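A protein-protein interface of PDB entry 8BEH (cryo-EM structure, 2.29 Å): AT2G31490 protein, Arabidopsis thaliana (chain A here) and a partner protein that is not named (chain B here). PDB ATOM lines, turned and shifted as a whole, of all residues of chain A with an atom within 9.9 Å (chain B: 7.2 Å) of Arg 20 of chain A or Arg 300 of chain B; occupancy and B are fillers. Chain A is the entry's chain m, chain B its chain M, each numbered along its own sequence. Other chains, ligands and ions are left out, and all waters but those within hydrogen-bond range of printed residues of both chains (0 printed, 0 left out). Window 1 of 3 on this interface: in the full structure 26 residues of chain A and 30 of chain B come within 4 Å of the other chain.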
ATOM      1  N   PHE A  12      -0.664  35.646  26.650  1.00  0.00           N
ATOM      2  CA  PHE A  12      -1.963  34.988  26.747  1.00  0.00           C
ATOM      3  C   PHE A  12      -2.463  34.524  25.383  1.00  0.00           C
ATOM      4  O   PHE A  12      -3.067  33.454  25.272  1.00  0.00           O
ATOM      5  CB  PHE A  12      -2.962  35.930  27.406  1.00  0.00           C
ATOM      6  CG  PHE A  12      -2.520  36.421  28.748  1.00  0.00           C
ATOM      7  CD1 PHE A  12      -2.783  35.681  29.886  1.00  0.00           C
ATOM      8  CD2 PHE A  12      -1.817  37.610  28.872  1.00  0.00           C
ATOM      9  CE1 PHE A  12      -2.377  36.126  31.125  1.00  0.00           C
ATOM     10  CE2 PHE A  12      -1.404  38.055  30.111  1.00  0.00           C
ATOM     11  CZ  PHE A  12      -1.682  37.310  31.236  1.00  0.00           C
ATOM     12  N   ILE A  13      -2.215  35.313  24.336  1.00  0.00           N
ATOM     13  CA  ILE A  13      -2.610  34.920  22.987  1.00  0.00           C
ATOM     14  C   ILE A  13      -1.843  33.677  22.546  1.00  0.00           C
ATOM     15  O   ILE A  13      -2.417  32.744  21.968  1.00  0.00           O
ATOM     16  CB  ILE A  13      -2.404  36.099  22.017  1.00  0.00           C
ATOM     17  CG1 ILE A  13      -3.390  37.220  22.341  1.00  0.00           C
ATOM     18  CG2 ILE A  13      -2.573  35.656  20.580  1.00  0.00           C
ATOM     19  CD1 ILE A  13      -3.108  38.501  21.599  1.00  0.00           C
ATOM     20  N   GLU A  14      -0.541  33.634  22.829  1.00  0.00           N
ATOM     21  CA  GLU A  14       0.244  32.449  22.499  1.00  0.00           C
ATOM     22  C   GLU A  14      -0.162  31.245  23.340  1.00  0.00           C
ATOM     23  O   GLU A  14      -0.174  30.118  22.837  1.00  0.00           O
ATOM     24  CB  GLU A  14       1.732  32.749  22.644  1.00  0.00           C
ATOM     25  CG  GLU A  14       2.153  33.926  21.807  1.00  0.00           C
ATOM     26  CD  GLU A  14       2.333  33.544  20.351  1.00  0.00           C
ATOM     27  OE1 GLU A  14       2.259  34.435  19.484  1.00  0.00           O
ATOM     28  OE2 GLU A  14       2.545  32.347  20.070  1.00  0.00           O
ATOM     29  N   ASP A  15      -0.497  31.458  24.616  1.00  0.00           N
ATOM     30  CA  ASP A  15      -1.004  30.359  25.433  1.00  0.00           C
ATOM     31  C   ASP A  15      -2.294  29.797  24.855  1.00  0.00           C
ATOM     32  O   ASP A  15      -2.471  28.579  24.777  1.00  0.00           O
ATOM     33  CB  ASP A  15      -1.232  30.827  26.871  1.00  0.00           C
ATOM     34  CG  ASP A  15       0.053  30.983  27.639  1.00  0.00           C
ATOM     35  OD1 ASP A  15       0.083  31.773  28.604  1.00  0.00           O
ATOM     36  OD2 ASP A  15       1.042  30.321  27.268  1.00  0.00           O
ATOM     37  N   TRP A  16      -3.201  30.681  24.438  1.00  0.00           N
ATOM     38  CA  TRP A  16      -4.447  30.272  23.800  1.00  0.00           C
ATOM     39  C   TRP A  16      -4.180  29.464  22.532  1.00  0.00           C
ATOM     40  O   TRP A  16      -4.758  28.385  22.332  1.00  0.00           O
ATOM     41  CB  TRP A  16      -5.256  31.533  23.506  1.00  0.00           C
ATOM     42  CG  TRP A  16      -6.580  31.385  22.852  1.00  0.00           C
ATOM     43  CD1 TRP A  16      -7.670  30.727  23.330  1.00  0.00           C
ATOM     44  CD2 TRP A  16      -6.964  31.947  21.599  1.00  0.00           C
ATOM     45  NE1 TRP A  16      -8.714  30.842  22.448  1.00  0.00           N
ATOM     46  CE2 TRP A  16      -8.304  31.588  21.374  1.00  0.00           C
ATOM     47  CE3 TRP A  16      -6.301  32.721  20.640  1.00  0.00           C
ATOM     48  CZ2 TRP A  16      -8.996  31.969  20.228  1.00  0.00           C
ATOM     49  CZ3 TRP A  16      -6.988  33.100  19.508  1.00  0.00           C
ATOM     50  CH2 TRP A  16      -8.322  32.725  19.312  1.00  0.00           C
ATOM     51  N   GLY A  17      -3.272  29.951  21.684  1.00  0.00           N
ATOM     52  CA  GLY A  17      -2.947  29.229  20.462  1.00  0.00           C
ATOM     53  C   GLY A  17      -2.338  27.861  20.715  1.00  0.00           C
ATOM     54  O   GLY A  17      -2.738  26.868  20.096  1.00  0.00           O
ATOM     55  N   SER A  18      -1.372  27.784  21.634  1.00  0.00           N
ATOM     56  CA  SER A  18      -0.734  26.505  21.926  1.00  0.00           C
ATOM     57  C   SER A  18      -1.702  25.531  22.585  1.00  0.00           C
ATOM     58  O   SER A  18      -1.627  24.325  22.332  1.00  0.00           O
ATOM     59  CB  SER A  18       0.504  26.711  22.801  1.00  0.00           C
ATOM     60  OG  SER A  18       0.252  27.610  23.862  1.00  0.00           O
ATOM     61  N   ALA A  19      -2.617  26.027  23.420  1.00  0.00           N
ATOM     62  CA  ALA A  19      -3.659  25.165  23.964  1.00  0.00           C
ATOM     63  C   ALA A  19      -4.529  24.604  22.849  1.00  0.00           C
ATOM     64  O   ALA A  19      -4.914  23.430  22.883  1.00  0.00           O
ATOM     65  CB  ALA A  19      -4.509  25.933  24.973  1.00  0.00           C
ATOM     66  N   ARG A  20      -4.795  25.427  21.831  1.00  0.00           N
ATOM     67  CA  ARG A  20      -5.580  24.952  20.660  1.00  0.00           C
ATOM     68  C   ARG A  20      -4.795  23.848  19.943  1.00  0.00           C
ATOM     69  O   ARG A  20      -5.429  22.856  19.528  1.00  0.00           O
ATOM     70  CB  ARG A  20      -5.885  26.121  19.717  1.00  0.00           C
ATOM     71  CG  ARG A  20      -6.728  25.747  18.507  1.00  0.00           C
ATOM     72  CD  ARG A  20      -8.057  25.113  18.874  1.00  0.00           C
ATOM     73  NE  ARG A  20      -8.870  25.958  19.741  1.00  0.00           N
ATOM     74  CZ  ARG A  20      -9.686  26.921  19.325  1.00  0.00           C
ATOM     75  NH1 ARG A  20      -9.808  27.186  18.036  1.00  0.00           N
ATOM     76  NH2 ARG A  20     -10.372  27.624  20.206  1.00  0.00           N
ATOM     77  N   GLU A  21      -3.471  24.001  19.818  1.00  0.00           N
ATOM     78  CA  GLU A  21      -2.683  23.019  19.076  1.00  0.00           C
ATOM     79  C   GLU A  21      -2.497  21.690  19.807  1.00  0.00           C
ATOM     80  O   GLU A  21      -2.039  20.729  19.183  1.00  0.00           O
ATOM     81  CB  GLU A  21      -1.299  23.577  18.726  1.00  0.00           C
ATOM     82  CG  GLU A  21      -1.312  24.874  17.958  1.00  0.00           C
ATOM     83  CD  GLU A  21      -0.239  25.839  18.424  1.00  0.00           C
ATOM     84  OE1 GLU A  21      -0.278  27.013  18.008  1.00  0.00           O
ATOM     85  OE2 GLU A  21       0.646  25.427  19.200  1.00  0.00           O
ATOM     86  N   ASN A  22      -2.831  21.597  21.089  1.00  0.00           N
ATOM     87  CA  ASN A  22      -2.535  20.407  21.877  1.00  0.00           C
ATOM     88  C   ASN A  22      -3.782  19.848  22.549  1.00  0.00           C
ATOM     89  O   ASN A  22      -3.737  19.352  23.675  1.00  0.00           O
ATOM     90  CB  ASN A  22      -1.448  20.708  22.904  1.00  0.00           C
ATOM     91  CG  ASN A  22      -0.167  21.182  22.260  1.00  0.00           C
ATOM     92  OD1 ASN A  22       0.318  22.276  22.538  1.00  0.00           O
ATOM     93  ND2 ASN A  22       0.383  20.363  21.379  1.00  0.00           N
ATOM     94  N   LEU A  23      -4.910  19.895  21.840  1.00  0.00           N
ATOM     95  CA  LEU A  23      -6.180  19.485  22.427  1.00  0.00           C
ATOM     96  C   LEU A  23      -6.234  17.986  22.703  1.00  0.00           C
ATOM     97  O   LEU A  23      -6.916  17.559  23.639  1.00  0.00           O
ATOM     98  CB  LEU A  23      -7.325  19.902  21.505  1.00  0.00           C
ATOM     99  CG  LEU A  23      -8.626  20.361  22.153  1.00  0.00           C
ATOM    100  CD1 LEU A  23      -8.346  21.351  23.272  1.00  0.00           C
ATOM    101  CD2 LEU A  23      -9.543  20.978  21.103  1.00  0.00           C
ATOM    102  N   GLU A  24      -5.519  17.178  21.917  1.00  0.00           N
ATOM    103  CA  GLU A  24      -5.623  15.727  22.041  1.00  0.00           C
ATOM    104  C   GLU A  24      -5.165  15.225  23.404  1.00  0.00           C
ATOM    105  O   GLU A  24      -5.598  14.152  23.832  1.00  0.00           O
ATOM    106  CB  GLU A  24      -4.816  15.037  20.936  1.00  0.00           C
ATOM    107  CG  GLU A  24      -3.324  15.379  20.900  1.00  0.00           C
ATOM    108  CD  GLU A  24      -3.021  16.737  20.301  1.00  0.00           C
ATOM    109  OE1 GLU A  24      -3.965  17.473  19.948  1.00  0.00           O
ATOM    110  OE2 GLU A  24      -1.826  17.073  20.179  1.00  0.00           O
ATOM    111  N   HIS A  25      -4.314  15.977  24.098  1.00  0.00           N
ATOM    112  CA  HIS A  25      -3.883  15.602  25.437  1.00  0.00           C
ATOM    113  C   HIS A  25      -4.978  15.769  26.477  1.00  0.00           C
ATOM    114  O   HIS A  25      -4.811  15.306  27.608  1.00  0.00           O
ATOM    115  CB  HIS A  25      -2.661  16.426  25.839  1.00  0.00           C
ATOM    116  CG  HIS A  25      -1.476  16.204  24.957  1.00  0.00           C
ATOM    117  ND1 HIS A  25      -0.890  17.217  24.232  1.00  0.00           N
ATOM    118  CD2 HIS A  25      -0.772  15.084  24.676  1.00  0.00           C
ATOM    119  CE1 HIS A  25       0.121  16.730  23.538  1.00  0.00           C
ATOM    120  NE2 HIS A  25       0.216  15.438  23.791  1.00  0.00           N
ATOM    121  N   ASN A  26      -6.093  16.399  26.123  1.00  0.00           N
ATOM    122  CA  ASN A  26      -7.160  16.675  27.067  1.00  0.00           C
ATOM    123  C   ASN A  26      -8.309  15.682  26.979  1.00  0.00           C
ATOM    124  O   ASN A  26      -9.150  15.655  27.882  1.00  0.00           O
ATOM    125  CB  ASN A  26      -7.696  18.089  26.837  1.00  0.00           C
ATOM    126  CG  ASN A  26      -6.694  19.149  27.214  1.00  0.00           C
ATOM    127  OD1 ASN A  26      -5.727  18.878  27.924  1.00  0.00           O
ATOM    128  ND2 ASN A  26      -6.915  20.368  26.737  1.00  0.00           N
ATOM    129  N   THR B 294     -15.750  19.090   8.134  1.00  0.00           N
ATOM    130  CA  THR B 294     -14.505  19.867   7.908  1.00  0.00           C
ATOM    131  C   THR B 294     -14.810  21.357   7.661  1.00  0.00           C
ATOM    132  O   THR B 294     -14.059  22.115   8.176  1.00  0.00           O
ATOM    133  CB  THR B 294     -13.534  19.164   6.940  1.00  0.00           C
ATOM    134  OG1 THR B 294     -13.913  19.274   5.567  1.00  0.00           O
ATOM    135  CG2 THR B 294     -13.311  17.709   7.307  1.00  0.00           C
ATOM    136  N   SER B 295     -15.865  21.711   6.925  1.00  0.00           N
ATOM    137  CA  SER B 295     -16.203  23.125   6.792  1.00  0.00           C
ATOM    138  C   SER B 295     -16.518  23.741   8.151  1.00  0.00           C
ATOM    139  O   SER B 295     -16.057  24.848   8.473  1.00  0.00           O
ATOM    140  CB  SER B 295     -17.387  23.298   5.838  1.00  0.00           C
ATOM    141  OG  SER B 295     -17.035  22.977   4.509  1.00  0.00           O
ATOM    142  N   LEU B 296     -17.283  23.022   8.976  1.00  0.00           N
ATOM    143  CA  LEU B 296     -17.605  23.547  10.296  1.00  0.00           C
ATOM    144  C   LEU B 296     -16.359  23.647  11.175  1.00  0.00           C
ATOM    145  O   LEU B 296     -16.213  24.603  11.943  1.00  0.00           O
ATOM    146  CB  LEU B 296     -18.684  22.683  10.946  1.00  0.00           C
ATOM    147  CG  LEU B 296     -20.081  22.995  10.395  1.00  0.00           C
ATOM    148  CD1 LEU B 296     -21.138  22.025  10.907  1.00  0.00           C
ATOM    149  CD2 LEU B 296     -20.480  24.443  10.655  1.00  0.00           C
ATOM    150  N   THR B 297     -15.421  22.678  11.103  1.00  0.00           N
ATOM    151  CA  THR B 297     -14.113  22.752  11.826  1.00  0.00           C
ATOM    152  C   THR B 297     -13.324  23.976  11.336  1.00  0.00           C
ATOM    153  O   THR B 297     -12.795  24.672  12.188  1.00  0.00           O
ATOM    154  CB  THR B 297     -13.295  21.446  11.734  1.00  0.00           C
ATOM    155  OG1 THR B 297     -13.871  20.405  12.512  1.00  0.00           O
ATOM    156  CG2 THR B 297     -11.847  21.620  12.148  1.00  0.00           C
ATOM    157  N   THR B 298     -13.311  24.211  10.027  1.00  0.00           N
ATOM    158  CA  THR B 298     -12.642  25.379   9.405  1.00  0.00           C
ATOM    159  C   THR B 298     -13.160  26.634  10.083  1.00  0.00           C
ATOM    160  O   THR B 298     -12.327  27.418  10.480  1.00  0.00           O
ATOM    161  CB  THR B 298     -12.724  25.398   7.842  1.00  0.00           C
ATOM    162  OG1 THR B 298     -12.428  24.097   7.342  1.00  0.00           O
ATOM    163  CG2 THR B 298     -11.859  26.439   7.172  1.00  0.00           C
ATOM    164  N   LEU B 299     -14.474  26.711  10.267  1.00  0.00           N
ATOM    165  CA  LEU B 299     -15.068  27.905  10.866  1.00  0.00           C
ATOM    166  C   LEU B 299     -14.442  28.269  12.214  1.00  0.00           C
ATOM    167  O   LEU B 299     -14.386  29.450  12.565  1.00  0.00           O
ATOM    168  CB  LEU B 299     -16.572  27.706  11.031  1.00  0.00           C
ATOM    169  CG  LEU B 299     -17.501  28.907  10.852  1.00  0.00           C
ATOM    170  CD1 LEU B 299     -17.078  29.784   9.697  1.00  0.00           C
ATOM    171  CD2 LEU B 299     -18.930  28.421  10.668  1.00  0.00           C
ATOM    172  N   ARG B 300     -13.966  27.288  12.979  1.00  0.00           N
ATOM    173  CA  ARG B 300     -13.502  27.527  14.340  1.00  0.00           C
ATOM    174  C   ARG B 300     -11.983  27.501  14.484  1.00  0.00           C
ATOM    175  O   ARG B 300     -11.484  27.416  15.608  1.00  0.00           O
ATOM    176  CB  ARG B 300     -14.134  26.510  15.292  1.00  0.00           C
ATOM    177  CG  ARG B 300     -15.640  26.656  15.453  1.00  0.00           C
ATOM    178  CD  ARG B 300     -16.038  28.077  15.819  1.00  0.00           C
ATOM    179  NE  ARG B 300     -15.418  28.512  17.065  1.00  0.00           N
ATOM    180  CZ  ARG B 300     -15.870  28.216  18.275  1.00  0.00           C
ATOM    181  NH1 ARG B 300     -16.960  27.487  18.446  1.00  0.00           N
ATOM    182  NH2 ARG B 300     -15.210  28.659  19.341  1.00  0.00           N
ATOM    183  N   GLN B 301     -11.251  27.573  13.394  1.00  0.00           N
ATOM    184  CA  GLN B 301      -9.763  27.593  13.395  1.00  0.00           C
ATOM    185  C   GLN B 301      -9.231  29.025  13.599  1.00  0.00           C
ATOM    186  O   GLN B 301      -9.854  29.962  13.233  1.00  0.00           O
ATOM    187  CB  GLN B 301      -9.224  26.760  12.216  1.00  0.00           C
ATOM    188  CG  GLN B 301      -9.709  25.330  12.174  1.00  0.00           C
ATOM    189  CD  GLN B 301      -9.031  24.486  13.220  1.00  0.00           C
ATOM    190  OE1 GLN B 301      -7.815  24.402  13.270  1.00  0.00           O
ATOM    191  NE2 GLN B 301      -9.822  23.877  14.080  1.00  0.00           N
ATOM    192  N   ILE B 302      -8.146  29.173  14.296  1.00  0.00           N
ATOM    193  CA  ILE B 302      -7.606  30.482  14.644  1.00  0.00           C
ATOM    194  C   ILE B 302      -6.270  30.767  13.980  1.00  0.00           C
ATOM    195  O   ILE B 302      -5.680  31.819  14.235  1.00  0.00           O
ATOM    196  CB  ILE B 302      -7.490  30.649  16.173  1.00  0.00           C
ATOM    197  CG1 ILE B 302      -6.444  29.683  16.736  1.00  0.00           C
ATOM    198  CG2 ILE B 302      -8.839  30.441  16.827  1.00  0.00           C
ATOM    199  CD1 ILE B 302      -6.277  29.761  18.221  1.00  0.00           C
ATOM    200  N   ASP B 303      -5.785  29.876  13.127  1.00  0.00           N
ATOM    201  CA  ASP B 303      -4.507  30.018  12.443  1.00  0.00           C
ATOM    202  C   ASP B 303      -4.793  30.157  10.951  1.00  0.00           C
ATOM    203  O   ASP B 303      -5.581  29.387  10.396  1.00  0.00           O
ATOM    204  CB  ASP B 303      -3.610  28.805  12.755  1.00  0.00           C
ATOM    205  CG  ASP B 303      -2.298  28.768  11.954  1.00  0.00           C
ATOM    206  OD1 ASP B 303      -1.306  28.262  12.514  1.00  0.00           O
ATOM    207  OD2 ASP B 303      -2.228  29.205  10.788  1.00  0.00           O
ATOM    208  N   ILE B 307      -6.714  27.443   8.530  1.00  0.00           N
ATOM    209  CA  ILE B 307      -8.006  27.732   7.840  1.00  0.00           C
ATOM    210  C   ILE B 307      -7.898  27.349   6.343  1.00  0.00           C
ATOM    211  O   ILE B 307      -8.663  26.524   5.926  1.00  0.00           O
ATOM    212  CB  ILE B 307      -8.564  29.159   8.123  1.00  0.00           C
ATOM    213  CG1 ILE B 307      -8.871  29.379   9.604  1.00  0.00           C
ATOM    214  CG2 ILE B 307      -9.743  29.497   7.225  1.00  0.00           C
ATOM    215  CD1 ILE B 307      -8.521  30.749  10.103  1.00  0.00           C
ATOM    216  N   LEU B 363      -1.346  33.551  13.869  1.00  0.00           N
ATOM    217  CA  LEU B 363      -2.535  33.737  14.685  1.00  0.00           C
ATOM    218  C   LEU B 363      -3.337  34.918  14.152  1.00  0.00           C
ATOM    219  O   LEU B 363      -2.811  36.027  14.019  1.00  0.00           O
ATOM    220  CB  LEU B 363      -2.129  33.956  16.141  1.00  0.00           C
ATOM    221  CG  LEU B 363      -1.684  32.682  16.873  1.00  0.00           C
ATOM    222  CD1 LEU B 363      -1.589  32.883  18.372  1.00  0.00           C
ATOM    223  CD2 LEU B 363      -2.606  31.516  16.549  1.00  0.00           C
ATOM    224  N   TYR B 428     -16.600  30.851   6.217  1.00  0.00           N
ATOM    225  CA  TYR B 428     -15.246  30.897   6.769  1.00  0.00           C
ATOM    226  C   TYR B 428     -14.328  31.781   5.929  1.00  0.00           C
ATOM    227  O   TYR B 428     -13.473  32.482   6.483  1.00  0.00           O
ATOM    228  CB  TYR B 428     -14.660  29.489   6.978  1.00  0.00           C
ATOM    229  CG  TYR B 428     -14.411  28.617   5.767  1.00  0.00           C
ATOM    230  CD1 TYR B 428     -13.467  28.960   4.810  1.00  0.00           C
ATOM    231  CD2 TYR B 428     -15.094  27.420   5.613  1.00  0.00           C
ATOM    232  CE1 TYR B 428     -13.241  28.160   3.720  1.00  0.00           C
ATOM    233  CE2 TYR B 428     -14.868  26.608   4.537  1.00  0.00           C
ATOM    234  CZ  TYR B 428     -13.945  26.983   3.586  1.00  0.00           C
ATOM    235  OH  TYR B 428     -13.720  26.172   2.501  1.00  0.00           O
ATOM    236  N   TRP B 431     -15.125  35.430   6.799  1.00  0.00           N
ATOM    237  CA  TRP B 431     -14.699  35.713   8.167  1.00  0.00           C
ATOM    238  C   TRP B 431     -13.185  35.884   8.246  1.00  0.00           C
ATOM    239  O   TRP B 431     -12.687  36.831   8.868  1.00  0.00           O
ATOM    240  CB  TRP B 431     -15.172  34.606   9.108  1.00  0.00           C
ATOM    241  CG  TRP B 431     -15.291  35.042  10.539  1.00  0.00           C
ATOM    242  CD1 TRP B 431     -15.268  36.325  11.013  1.00  0.00           C
ATOM    243  CD2 TRP B 431     -15.457  34.198  11.683  1.00  0.00           C
ATOM    244  NE1 TRP B 431     -15.401  36.328  12.376  1.00  0.00           N
ATOM    245  CE2 TRP B 431     -15.518  35.036  12.814  1.00  0.00           C
ATOM    246  CE3 TRP B 431     -15.552  32.815  11.863  1.00  0.00           C
ATOM    247  CZ2 TRP B 431     -15.675  34.537  14.107  1.00  0.00           C
ATOM    248  CZ3 TRP B 431     -15.710  32.321  13.146  1.00  0.00           C
ATOM    249  CH2 TRP B 431     -15.769  33.182  14.251  1.00  0.00           C
ATOM    250  N   ARG B 435     -11.376  39.456   9.224  1.00  0.00           N
ATOM    251  CA  ARG B 435     -10.558  39.538  10.429  1.00  0.00           C
ATOM    252  C   ARG B 435      -9.111  39.898  10.114  1.00  0.00           C
ATOM    253  O   ARG B 435      -8.427  40.482  10.959  1.00  0.00           O
ATOM    254  CB  ARG B 435     -10.631  38.226  11.209  1.00  0.00           C
ATOM    255  CG  ARG B 435     -11.883  38.108  12.066  1.00  0.00           C
ATOM    256  CD  ARG B 435     -11.951  36.776  12.767  1.00  0.00           C
ATOM    257  NE  ARG B 435     -12.274  35.691  11.849  1.00  0.00           N
ATOM    258  CZ  ARG B 435     -12.095  34.406  12.119  1.00  0.00           C
ATOM    259  NH1 ARG B 435     -11.607  34.008  13.283  1.00  0.00           N
ATOM    260  NH2 ARG B 435     -12.406  33.500  11.197  1.00  0.00           N
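The backbone carbonyl oxygen (O) of Arg 300 of chain B is in hydrogen-bond range of the guanidinium group (NH1) of Arg 20 of chain A (3.0 Å).
Ile 13 of chain A touches Leu 363 of chain B (CG2 to CD1, 3.7 Å). CG2 of Ile 302 of chain B touches CH2 of Trp 16 of chain A, at 3.4 Å. Ile 302 of chain B touches Arg 20 of chain A (CG2 to NH1, 3.6 Å).
Printed residues of chain B within 4 Å of Ile 13 of chain A: Leu 363. Printed residues of chain B within 4 Å of Trp 16 of chain A: Ile 302. Arg 20 of chain A touches two residues of chain B. Arg 300 of chain B touches just one residue of chain A: Arg 20. Gln 301 of chain B touches none of the printed residues of chain A. Printed residues of chain A within 4 Å of Ile 302 of chain B: Trp 16 and Arg 20. Asp 303 of chain B touches none of the printed residues of chain A. Printed residues of chain A within 4 Å of Leu 363 of chain B: Ile 13 (3.7 Å). The nearest residue of chain B that does not touch Arg 20 of chain A is Gln 301 of chain B (4.7 Å). The nearest residue of chain A that does not touch Arg 300 of chain B is Trp 16 of chain A (6.9 Å). The nearest printed residue of chain A that does not touch Ile 302 of chain B is Gly 17 of chain A (4.05 Å).
Along chain B the printed residues that touch a printed residue of chain A span positions 300 to 363. Of the 15 printed residues of chain A, 3 touch a printed residue of chain B.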
